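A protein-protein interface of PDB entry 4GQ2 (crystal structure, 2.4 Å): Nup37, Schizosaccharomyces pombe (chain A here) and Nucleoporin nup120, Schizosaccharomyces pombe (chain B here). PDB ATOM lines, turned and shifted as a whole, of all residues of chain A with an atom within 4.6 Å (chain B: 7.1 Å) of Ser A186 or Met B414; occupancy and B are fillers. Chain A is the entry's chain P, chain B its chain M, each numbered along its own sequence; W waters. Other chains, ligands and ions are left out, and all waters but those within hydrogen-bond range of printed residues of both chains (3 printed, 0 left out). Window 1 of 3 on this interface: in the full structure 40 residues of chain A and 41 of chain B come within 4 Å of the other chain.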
ATOM      1  N   PRO A 184      23.560 -11.928 -32.424  1.00  0.00           N
ATOM      2  CA  PRO A 184      24.296 -12.424 -31.265  1.00  0.00           C
ATOM      3  C   PRO A 184      23.570 -12.177 -29.947  1.00  0.00           C
ATOM      4  O   PRO A 184      22.832 -11.196 -29.814  1.00  0.00           O
ATOM      5  CB  PRO A 184      25.608 -11.625 -31.307  1.00  0.00           C
ATOM      6  CG  PRO A 184      25.395 -10.530 -32.315  1.00  0.00           C
ATOM      7  CD  PRO A 184      24.410 -11.089 -33.290  1.00  0.00           C
ATOM      8  N   LEU A 185      23.781 -13.072 -28.986  1.00  0.00           N
ATOM      9  CA  LEU A 185      23.281 -12.882 -27.621  1.00  0.00           C
ATOM     10  C   LEU A 185      24.477 -12.914 -26.689  1.00  0.00           C
ATOM     11  O   LEU A 185      25.567 -13.341 -27.093  1.00  0.00           O
ATOM     12  CB  LEU A 185      22.289 -13.986 -27.247  1.00  0.00           C
ATOM     13  CG  LEU A 185      21.096 -14.225 -28.176  1.00  0.00           C
ATOM     14  CD1 LEU A 185      20.354 -15.469 -27.735  1.00  0.00           C
ATOM     15  CD2 LEU A 185      20.165 -13.019 -28.215  1.00  0.00           C
ATOM     16  N   SER A 186      24.285 -12.475 -25.449  1.00  0.00           N
ATOM     17  CA  SER A 186      25.407 -12.372 -24.518  1.00  0.00           C
ATOM     18  C   SER A 186      25.680 -13.686 -23.795  1.00  0.00           C
ATOM     19  O   SER A 186      26.687 -13.826 -23.108  1.00  0.00           O
ATOM     20  CB  SER A 186      25.182 -11.254 -23.508  1.00  0.00           C
ATOM     21  OG  SER A 186      24.575 -11.775 -22.327  1.00  0.00           O
ATOM     22  N   SER A 187      24.770 -14.638 -23.934  1.00  0.00           N
ATOM     23  CA  SER A 187      24.924 -15.957 -23.319  1.00  0.00           C
ATOM     24  C   SER A 187      23.921 -16.904 -23.978  1.00  0.00           C
ATOM     25  O   SER A 187      23.254 -16.512 -24.941  1.00  0.00           O
ATOM     26  CB  SER A 187      24.785 -15.889 -21.786  1.00  0.00           C
ATOM     27  OG  SER A 187      23.460 -15.620 -21.376  1.00  0.00           O
ATOM     28  N   GLU A 206      17.884 -15.049 -21.961  1.00  0.00           N
ATOM     29  CA  GLU A 206      19.235 -15.627 -21.938  1.00  0.00           C
ATOM     30  C   GLU A 206      19.491 -16.397 -20.655  1.00  0.00           C
ATOM     31  O   GLU A 206      18.809 -16.183 -19.655  1.00  0.00           O
ATOM     32  CB  GLU A 206      20.272 -14.521 -22.048  1.00  0.00           C
ATOM     33  CG  GLU A 206      20.420 -13.936 -23.442  1.00  0.00           C
ATOM     34  CD  GLU A 206      21.554 -12.950 -23.515  1.00  0.00           C
ATOM     35  OE1 GLU A 206      22.546 -13.133 -22.766  1.00  0.00           O
ATOM     36  OE2 GLU A 206      21.452 -11.989 -24.308  1.00  0.00           O
ATOM     37  N   ASN A 208      21.856 -16.174 -18.461  1.00  0.00           N
ATOM     38  CA  ASN A 208      22.261 -15.272 -17.389  1.00  0.00           C
ATOM     39  C   ASN A 208      21.121 -14.357 -16.876  1.00  0.00           C
ATOM     40  O   ASN A 208      21.349 -13.464 -16.064  1.00  0.00           O
ATOM     41  CB  ASN A 208      23.462 -14.439 -17.847  1.00  0.00           C
ATOM     42  CG  ASN A 208      23.110 -13.473 -18.976  1.00  0.00           C
ATOM     43  OD1 ASN A 208      21.938 -13.183 -19.219  1.00  0.00           O
ATOM     44  ND2 ASN A 208      24.131 -12.949 -19.651  1.00  0.00           N
ATOM     45  N   ARG A 212      15.279  -9.804 -23.146  1.00  0.00           N
ATOM     46  CA  ARG A 212      15.389  -8.806 -24.199  1.00  0.00           C
ATOM     47  C   ARG A 212      14.157  -8.784 -25.092  1.00  0.00           C
ATOM     48  O   ARG A 212      13.696  -9.832 -25.545  1.00  0.00           O
ATOM     49  CB  ARG A 212      16.651  -9.050 -25.029  1.00  0.00           C
ATOM     50  CG  ARG A 212      17.825  -9.589 -24.224  1.00  0.00           C
ATOM     51  CD  ARG A 212      19.115  -8.892 -24.602  1.00  0.00           C
ATOM     52  NE  ARG A 212      20.297  -9.561 -24.067  1.00  0.00           N
ATOM     53  CZ  ARG A 212      21.057  -9.096 -23.082  1.00  0.00           C
ATOM     54  NH1 ARG A 212      20.771  -7.941 -22.496  1.00  0.00           N
ATOM     55  NH2 ARG A 212      22.119  -9.792 -22.685  1.00  0.00           N
ATOM     56  N   TRP A 235      16.931  -3.717 -30.575  1.00  0.00           N
ATOM     57  CA  TRP A 235      16.912  -4.161 -29.184  1.00  0.00           C
ATOM     58  C   TRP A 235      16.253  -3.130 -28.323  1.00  0.00           C
ATOM     59  O   TRP A 235      16.906  -2.215 -27.813  1.00  0.00           O
ATOM     60  CB  TRP A 235      18.335  -4.463 -28.710  1.00  0.00           C
ATOM     61  CG  TRP A 235      18.896  -5.655 -29.432  1.00  0.00           C
ATOM     62  CD1 TRP A 235      19.839  -5.664 -30.457  1.00  0.00           C
ATOM     63  CD2 TRP A 235      18.514  -7.058 -29.247  1.00  0.00           C
ATOM     64  NE1 TRP A 235      20.079  -6.942 -30.888  1.00  0.00           N
ATOM     65  CE2 TRP A 235      19.315  -7.829 -30.205  1.00  0.00           C
ATOM     66  CE3 TRP A 235      17.632  -7.732 -28.403  1.00  0.00           C
ATOM     67  CZ2 TRP A 235      19.220  -9.210 -30.295  1.00  0.00           C
ATOM     68  CZ3 TRP A 235      17.547  -9.126 -28.506  1.00  0.00           C
ATOM     69  CH2 TRP A 235      18.323  -9.845 -29.429  1.00  0.00           C
ATOM     70  N   THR A 238      16.196  -4.175 -22.357  1.00  0.00           N
ATOM     71  CA  THR A 238      16.683  -5.262 -21.546  1.00  0.00           C
ATOM     72  C   THR A 238      16.053  -5.147 -20.167  1.00  0.00           C
ATOM     73  O   THR A 238      16.055  -4.075 -19.566  1.00  0.00           O
ATOM     74  CB  THR A 238      18.220  -5.274 -21.447  1.00  0.00           C
ATOM     75  OG1 THR A 238      18.776  -5.656 -22.718  1.00  0.00           O
ATOM     76  CG2 THR A 238      18.704  -6.258 -20.347  1.00  0.00           C
ATOM     77  N   VAL B 410      25.569   3.326 -27.020  1.00  0.00           N
ATOM     78  CA  VAL B 410      24.479   2.441 -26.668  1.00  0.00           C
ATOM     79  C   VAL B 410      24.516   1.213 -27.586  1.00  0.00           C
ATOM     80  O   VAL B 410      24.489   1.361 -28.806  1.00  0.00           O
ATOM     81  CB  VAL B 410      23.128   3.194 -26.745  1.00  0.00           C
ATOM     82  CG1 VAL B 410      21.958   2.228 -26.823  1.00  0.00           C
ATOM     83  CG2 VAL B 410      22.970   4.123 -25.547  1.00  0.00           C
ATOM     84  N   PRO B 411      24.613   0.000 -26.996  1.00  0.00           N
ATOM     85  CA  PRO B 411      24.751  -1.228 -27.780  1.00  0.00           C
ATOM     86  C   PRO B 411      23.622  -1.438 -28.779  1.00  0.00           C
ATOM     87  O   PRO B 411      22.446  -1.316 -28.423  1.00  0.00           O
ATOM     88  CB  PRO B 411      24.723  -2.352 -26.726  1.00  0.00           C
ATOM     89  CG  PRO B 411      24.507  -1.695 -25.399  1.00  0.00           C
ATOM     90  CD  PRO B 411      24.817  -0.241 -25.552  1.00  0.00           C
ATOM     91  N   THR B 412      23.991  -1.778 -30.011  1.00  0.00           N
ATOM     92  CA  THR B 412      23.028  -2.009 -31.088  1.00  0.00           C
ATOM     93  C   THR B 412      22.937  -3.498 -31.371  1.00  0.00           C
ATOM     94  O   THR B 412      22.074  -3.948 -32.125  1.00  0.00           O
ATOM     95  CB  THR B 412      23.442  -1.269 -32.377  1.00  0.00           C
ATOM     96  OG1 THR B 412      24.819  -1.551 -32.669  1.00  0.00           O
ATOM     97  CG2 THR B 412      23.256   0.237 -32.213  1.00  0.00           C
ATOM     98  N   ASN B 413      23.856  -4.248 -30.769  1.00  0.00           N
ATOM     99  CA  ASN B 413      23.842  -5.700 -30.798  1.00  0.00           C
ATOM    100  C   ASN B 413      24.098  -6.203 -29.375  1.00  0.00           C
ATOM    101  O   ASN B 413      24.592  -5.445 -28.531  1.00  0.00           O
ATOM    102  CB  ASN B 413      24.898  -6.219 -31.775  1.00  0.00           C
ATOM    103  CG  ASN B 413      26.299  -6.148 -31.206  1.00  0.00           C
ATOM    104  OD1 ASN B 413      26.713  -7.017 -30.440  1.00  0.00           O
ATOM    105  ND2 ASN B 413      27.037  -5.118 -31.576  1.00  0.00           N
ATOM    106  N   MET B 414      23.783  -7.469 -29.105  1.00  0.00           N
ATOM    107  CA  MET B 414      23.876  -7.982 -27.733  1.00  0.00           C
ATOM    108  C   MET B 414      25.066  -8.908 -27.461  1.00  0.00           C
ATOM    109  O   MET B 414      25.102  -9.562 -26.420  1.00  0.00           O
ATOM    110  CB  MET B 414      22.557  -8.635 -27.290  1.00  0.00           C
ATOM    111  CG  MET B 414      21.361  -7.683 -27.226  1.00  0.00           C
ATOM    112  SD  MET B 414      21.383  -6.528 -25.833  1.00  0.00           S
ATOM    113  CE  MET B 414      21.856  -4.987 -26.628  1.00  0.00           C
ATOM    114  N   SER B 415      26.045  -8.928 -28.367  1.00  0.00           N
ATOM    115  CA  SER B 415      27.260  -9.767 -28.205  1.00  0.00           C
ATOM    116  C   SER B 415      27.954  -9.613 -26.856  1.00  0.00           C
ATOM    117  O   SER B 415      28.449 -10.589 -26.312  1.00  0.00           O
ATOM    118  CB  SER B 415      28.265  -9.525 -29.327  1.00  0.00           C
ATOM    119  OG  SER B 415      28.679  -8.173 -29.340  1.00  0.00           O
ATOM    120  N   SER B 416      27.967  -8.396 -26.314  1.00  0.00           N
ATOM    121  CA  SER B 416      28.454  -8.155 -24.948  1.00  0.00           C
ATOM    122  C   SER B 416      27.343  -7.659 -24.003  1.00  0.00           C
ATOM    123  O   SER B 416      27.620  -7.072 -22.950  1.00  0.00           O
ATOM    124  CB  SER B 416      29.619  -7.162 -24.963  1.00  0.00           C
ATOM    125  OG  SER B 416      30.793  -7.761 -25.495  1.00  0.00           O
ATOM    126  N   GLY B 417      26.088  -7.901 -24.375  1.00  0.00           N
ATOM    127  CA  GLY B 417      24.955  -7.524 -23.529  1.00  0.00           C
ATOM    128  C   GLY B 417      24.572  -6.062 -23.635  1.00  0.00           C
ATOM    129  O   GLY B 417      25.048  -5.348 -24.524  1.00  0.00           O
ATOM    130  N   ASP B 418      23.719  -5.613 -22.718  1.00  0.00           N
ATOM    131  CA  ASP B 418      23.163  -4.259 -22.782  1.00  0.00           C
ATOM    132  C   ASP B 418      23.852  -3.313 -21.790  1.00  0.00           C
ATOM    133  O   ASP B 418      24.826  -3.691 -21.139  1.00  0.00           O
ATOM    134  CB  ASP B 418      21.648  -4.303 -22.559  1.00  0.00           C
ATOM    135  CG  ASP B 418      20.882  -3.254 -23.386  1.00  0.00           C
ATOM    136  OD1 ASP B 418      21.451  -2.194 -23.748  1.00  0.00           O
ATOM    137  OD2 ASP B 418      19.692  -3.502 -23.673  1.00  0.00           O
ATOM    138  N   ILE B 419      23.332  -2.090 -21.685  1.00  0.00           N
ATOM    139  CA  ILE B 419      23.946  -0.995 -20.932  1.00  0.00           C
ATOM    140  C   ILE B 419      24.338  -1.366 -19.507  1.00  0.00           C
ATOM    141  O   ILE B 419      25.471  -1.133 -19.089  1.00  0.00           O
ATOM    142  CB  ILE B 419      23.029   0.254 -20.924  1.00  0.00           C
ATOM    143  CG1 ILE B 419      22.815   0.755 -22.351  1.00  0.00           C
ATOM    144  CG2 ILE B 419      23.615   1.383 -20.083  1.00  0.00           C
ATOM    145  CD1 ILE B 419      21.728   1.797 -22.478  1.00  0.00           C
ATOM    146  N   GLU B 421      24.602  -4.434 -17.962  1.00  0.00           N
ATOM    147  CA  GLU B 421      25.627  -5.488 -17.974  1.00  0.00           C
ATOM    148  C   GLU B 421      27.026  -4.922 -18.193  1.00  0.00           C
ATOM    149  O   GLU B 421      27.950  -5.238 -17.438  1.00  0.00           O
ATOM    150  CB  GLU B 421      25.332  -6.533 -19.043  1.00  0.00           C
ATOM    151  CG  GLU B 421      24.048  -7.316 -18.829  1.00  0.00           C
ATOM    152  CD  GLU B 421      23.402  -7.709 -20.148  1.00  0.00           C
ATOM    153  OE1 GLU B 421      22.502  -6.970 -20.645  1.00  0.00           O
ATOM    154  OE2 GLU B 421      23.810  -8.754 -20.695  1.00  0.00           O
ATOM    155  N   ILE B 422      27.172  -4.067 -19.204  1.00  0.00           N
ATOM    156  CA  ILE B 422      28.484  -3.515 -19.575  1.00  0.00           C
ATOM    157  C   ILE B 422      29.052  -2.580 -18.511  1.00  0.00           C
ATOM    158  O   ILE B 422      30.223  -2.708 -18.128  1.00  0.00           O
ATOM    159  CB  ILE B 422      28.448  -2.808 -20.945  1.00  0.00           C
ATOM    160  CG1 ILE B 422      28.055  -3.803 -22.050  1.00  0.00           C
ATOM    161  CG2 ILE B 422      29.791  -2.155 -21.242  1.00  0.00           C
ATOM    162  CD1 ILE B 422      27.579  -3.145 -23.333  1.00  0.00           C
ATOM    163  N   LYS B 496      17.381   4.385 -22.728  1.00  0.00           N
ATOM    164  CA  LYS B 496      18.765   3.949 -22.890  1.00  0.00           C
ATOM    165  C   LYS B 496      19.738   5.056 -22.513  1.00  0.00           C
ATOM    166  O   LYS B 496      20.635   4.840 -21.698  1.00  0.00           O
ATOM    167  CB  LYS B 496      19.021   3.454 -24.315  1.00  0.00           C
ATOM    168  CG  LYS B 496      18.285   2.162 -24.648  1.00  0.00           C
ATOM    169  CD  LYS B 496      18.477   1.778 -26.106  1.00  0.00           C
ATOM    170  CE  LYS B 496      17.543   0.653 -26.521  1.00  0.00           C
ATOM    171  NZ  LYS B 496      17.882  -0.652 -25.880  1.00  0.00           N
ATOM    172  N   SER B 594      33.236  -5.876 -30.109  1.00  0.00           N
ATOM    173  CA  SER B 594      32.377  -6.804 -29.404  1.00  0.00           C
ATOM    174  C   SER B 594      31.787  -7.811 -30.389  1.00  0.00           C
ATOM    175  O   SER B 594      31.612  -8.990 -30.057  1.00  0.00           O
ATOM    176  CB  SER B 594      31.295  -6.030 -28.649  1.00  0.00           C
ATOM    177  OG  SER B 594      30.396  -6.905 -28.009  1.00  0.00           O
ATOM    178  N   GLU B 595      31.512  -7.348 -31.605  1.00  0.00           N
ATOM    179  CA  GLU B 595      30.984  -8.216 -32.658  1.00  0.00           C
ATOM    180  C   GLU B 595      32.072  -9.138 -33.206  1.00  0.00           C
ATOM    181  O   GLU B 595      31.813 -10.306 -33.524  1.00  0.00           O
ATOM    182  CB  GLU B 595      30.360  -7.388 -33.788  1.00  0.00           C
ATOM    183  CG  GLU B 595      29.115  -6.623 -33.362  1.00  0.00           C
ATOM    184  CD  GLU B 595      28.400  -5.940 -34.512  1.00  0.00           C
ATOM    185  OE1 GLU B 595      28.847  -4.849 -34.934  1.00  0.00           O
ATOM    186  OE2 GLU B 595      27.371  -6.484 -34.975  1.00  0.00           O
ATOM    187  N   TYR B 598      32.796 -12.015 -30.766  1.00  0.00           N
ATOM    188  CA  TYR B 598      31.720 -12.988 -30.914  1.00  0.00           C
ATOM    189  C   TYR B 598      31.920 -13.872 -32.152  1.00  0.00           C
ATOM    190  O   TYR B 598      31.693 -15.068 -32.092  1.00  0.00           O
ATOM    191  CB  TYR B 598      30.359 -12.276 -30.975  1.00  0.00           C
ATOM    192  CG  TYR B 598      29.214 -13.207 -31.306  1.00  0.00           C
ATOM    193  CD1 TYR B 598      28.929 -13.544 -32.630  1.00  0.00           C
ATOM    194  CD2 TYR B 598      28.423 -13.768 -30.293  1.00  0.00           C
ATOM    195  CE1 TYR B 598      27.889 -14.407 -32.943  1.00  0.00           C
ATOM    196  CE2 TYR B 598      27.376 -14.629 -30.598  1.00  0.00           C
ATOM    197  CZ  TYR B 598      27.114 -14.942 -31.920  1.00  0.00           C
ATOM    198  OH  TYR B 598      26.079 -15.790 -32.231  1.00  0.00           O
ATOM    199  N   ARG B 601      34.990 -16.102 -31.315  1.00  0.00           N
ATOM    200  CA  ARG B 601      34.482 -17.116 -30.394  1.00  0.00           C
ATOM    201  C   ARG B 601      33.811 -18.226 -31.192  1.00  0.00           C
ATOM    202  O   ARG B 601      34.092 -19.407 -30.992  1.00  0.00           O
ATOM    203  CB  ARG B 601      33.468 -16.467 -29.457  1.00  0.00           C
ATOM    204  CG  ARG B 601      33.323 -17.090 -28.083  1.00  0.00           C
ATOM    205  CD  ARG B 601      32.336 -16.274 -27.264  1.00  0.00           C
ATOM    206  NE  ARG B 601      32.790 -14.891 -27.100  1.00  0.00           N
ATOM    207  CZ  ARG B 601      32.017 -13.813 -27.229  1.00  0.00           C
ATOM    208  NH1 ARG B 601      30.738 -13.937 -27.544  1.00  0.00           N
ATOM    209  NH2 ARG B 601      32.532 -12.602 -27.062  1.00  0.00           N
HETATM  210  O   HOH W   1      28.260 -14.217 -26.799  1.00  0.00           O
HETATM  211  O   HOH W   2      22.460  -8.754 -31.257  1.00  0.00           O
HETATM  212  O   HOH W   3      26.184 -10.188 -20.175  1.00  0.00           O
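OG1 of Thr A238 is in hydrogen-bond range of OD2 of Asp B418, 2.5 Å away.
The backbone carbonyl oxygen of Trp A235 is in hydrogen-bond range of the side-chain amino group of Lys B496 (2.7 Å).
The side-chain sulfur of Met B414 sits close to the guanidinium group of Arg A212 (3.7 Å).
The side-chain carboxylate (OE1) of Glu B421 lies within salt-bridge range of the guanidinium group (NH1) of Arg A212, 2.7 Å away.
The backbone carbonyl oxygen (O) of Met B414 is in hydrogen-bond range of the backbone NH (N) of Ser A186, 3.2 Å away.
OG of Ser B594 lies within hydrogen-bond range of OG of Ser B415.
OD1 of Asn B413 lies within hydrogen-bond range of OG of Ser B415 (2.5 Å).
The guanidinium group of Arg A212 lies within hydrogen-bond range of the side-chain hydroxyl of Ser A186 (3.2 Å).
OG of Ser A186 sits at hydrogen-bond distance from OE1 of Glu A206, 2.5 Å away.
OE1 of Glu B421 sits at hydrogen-bond distance from N of Asp B418, at 2.8 Å.
OG1 of Thr A238 sits at hydrogen-bond distance from NH1 of Arg A212, 3.0 Å away.
Among the printed residues, merely in contact across the chains: Pro A184 with Met B414, Pro A184 with Ser B415, Pro A184 with Tyr B598, Leu A185 with Met B414, Ser A186 with Ser B415, Ser A186 with Gly B417, Ser A186 with Glu B421, Arg A212 with Gly B417, Arg A212 with Asp B418, Trp A235 with Thr B412, Trp A235 with Asn B413, Trp A235 with Met B414 and Thr A238 with Glu B421.
Printed residues of chain A within 4 Å of Met B414: Pro A184, Leu A185, Ser A186, Arg A212 and Trp A235.
Printed residues of chain A within 4 Å of Tyr B598: Pro A184 (3.6 Å).
Of the printed residues of chain B, Leu A185 touches Met B414 (3.4 Å).
Printed residues of chain A within 4 Å of Ser B415: Pro A184 (3.9 Å) and Ser A186 (3.96 Å).
The nearest printed residue of chain A that does not touch Ser B415 is Leu A185 (4.1 Å).
Hydrophobic or aromatic side chains of chain B within 4 Å of the printed part of chain A: Met B414 and Tyr B598.
Of the 9 printed residues of chain A, 6 touch a printed residue of chain B.
Printed residues of chain A that touch a printed residue of chain B: Pro A184, Leu A185, Ser A186, Arg A212, Trp A235 and Thr A238.
Among the printed residues, 18 pairs touch across the chains.
Among the printed residues, Asp or Glu carboxylates within 4 Å of a Lys or Arg side-chain nitrogen of the other chain: Arg A212 with Glu B421.
Water W1 lies within hydrogen-bond range of the guanidinium group (NH1) of Arg B601 (2.6 Å) and the backbone carbonyl oxygen (O) of Leu A185 (2.8 Å).
Water W3 lies within hydrogen-bond range of OE2 of Glu B421, OG of Ser A186 and ND2 of Asn A208.
Water W2 lies within hydrogen-bond range of the backbone NH of Met B414 (2.8 Å), the backbone carbonyl oxygen of Pro A184 (2.9 Å) and the indole nitrogen of Trp A235 (3.0 Å).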
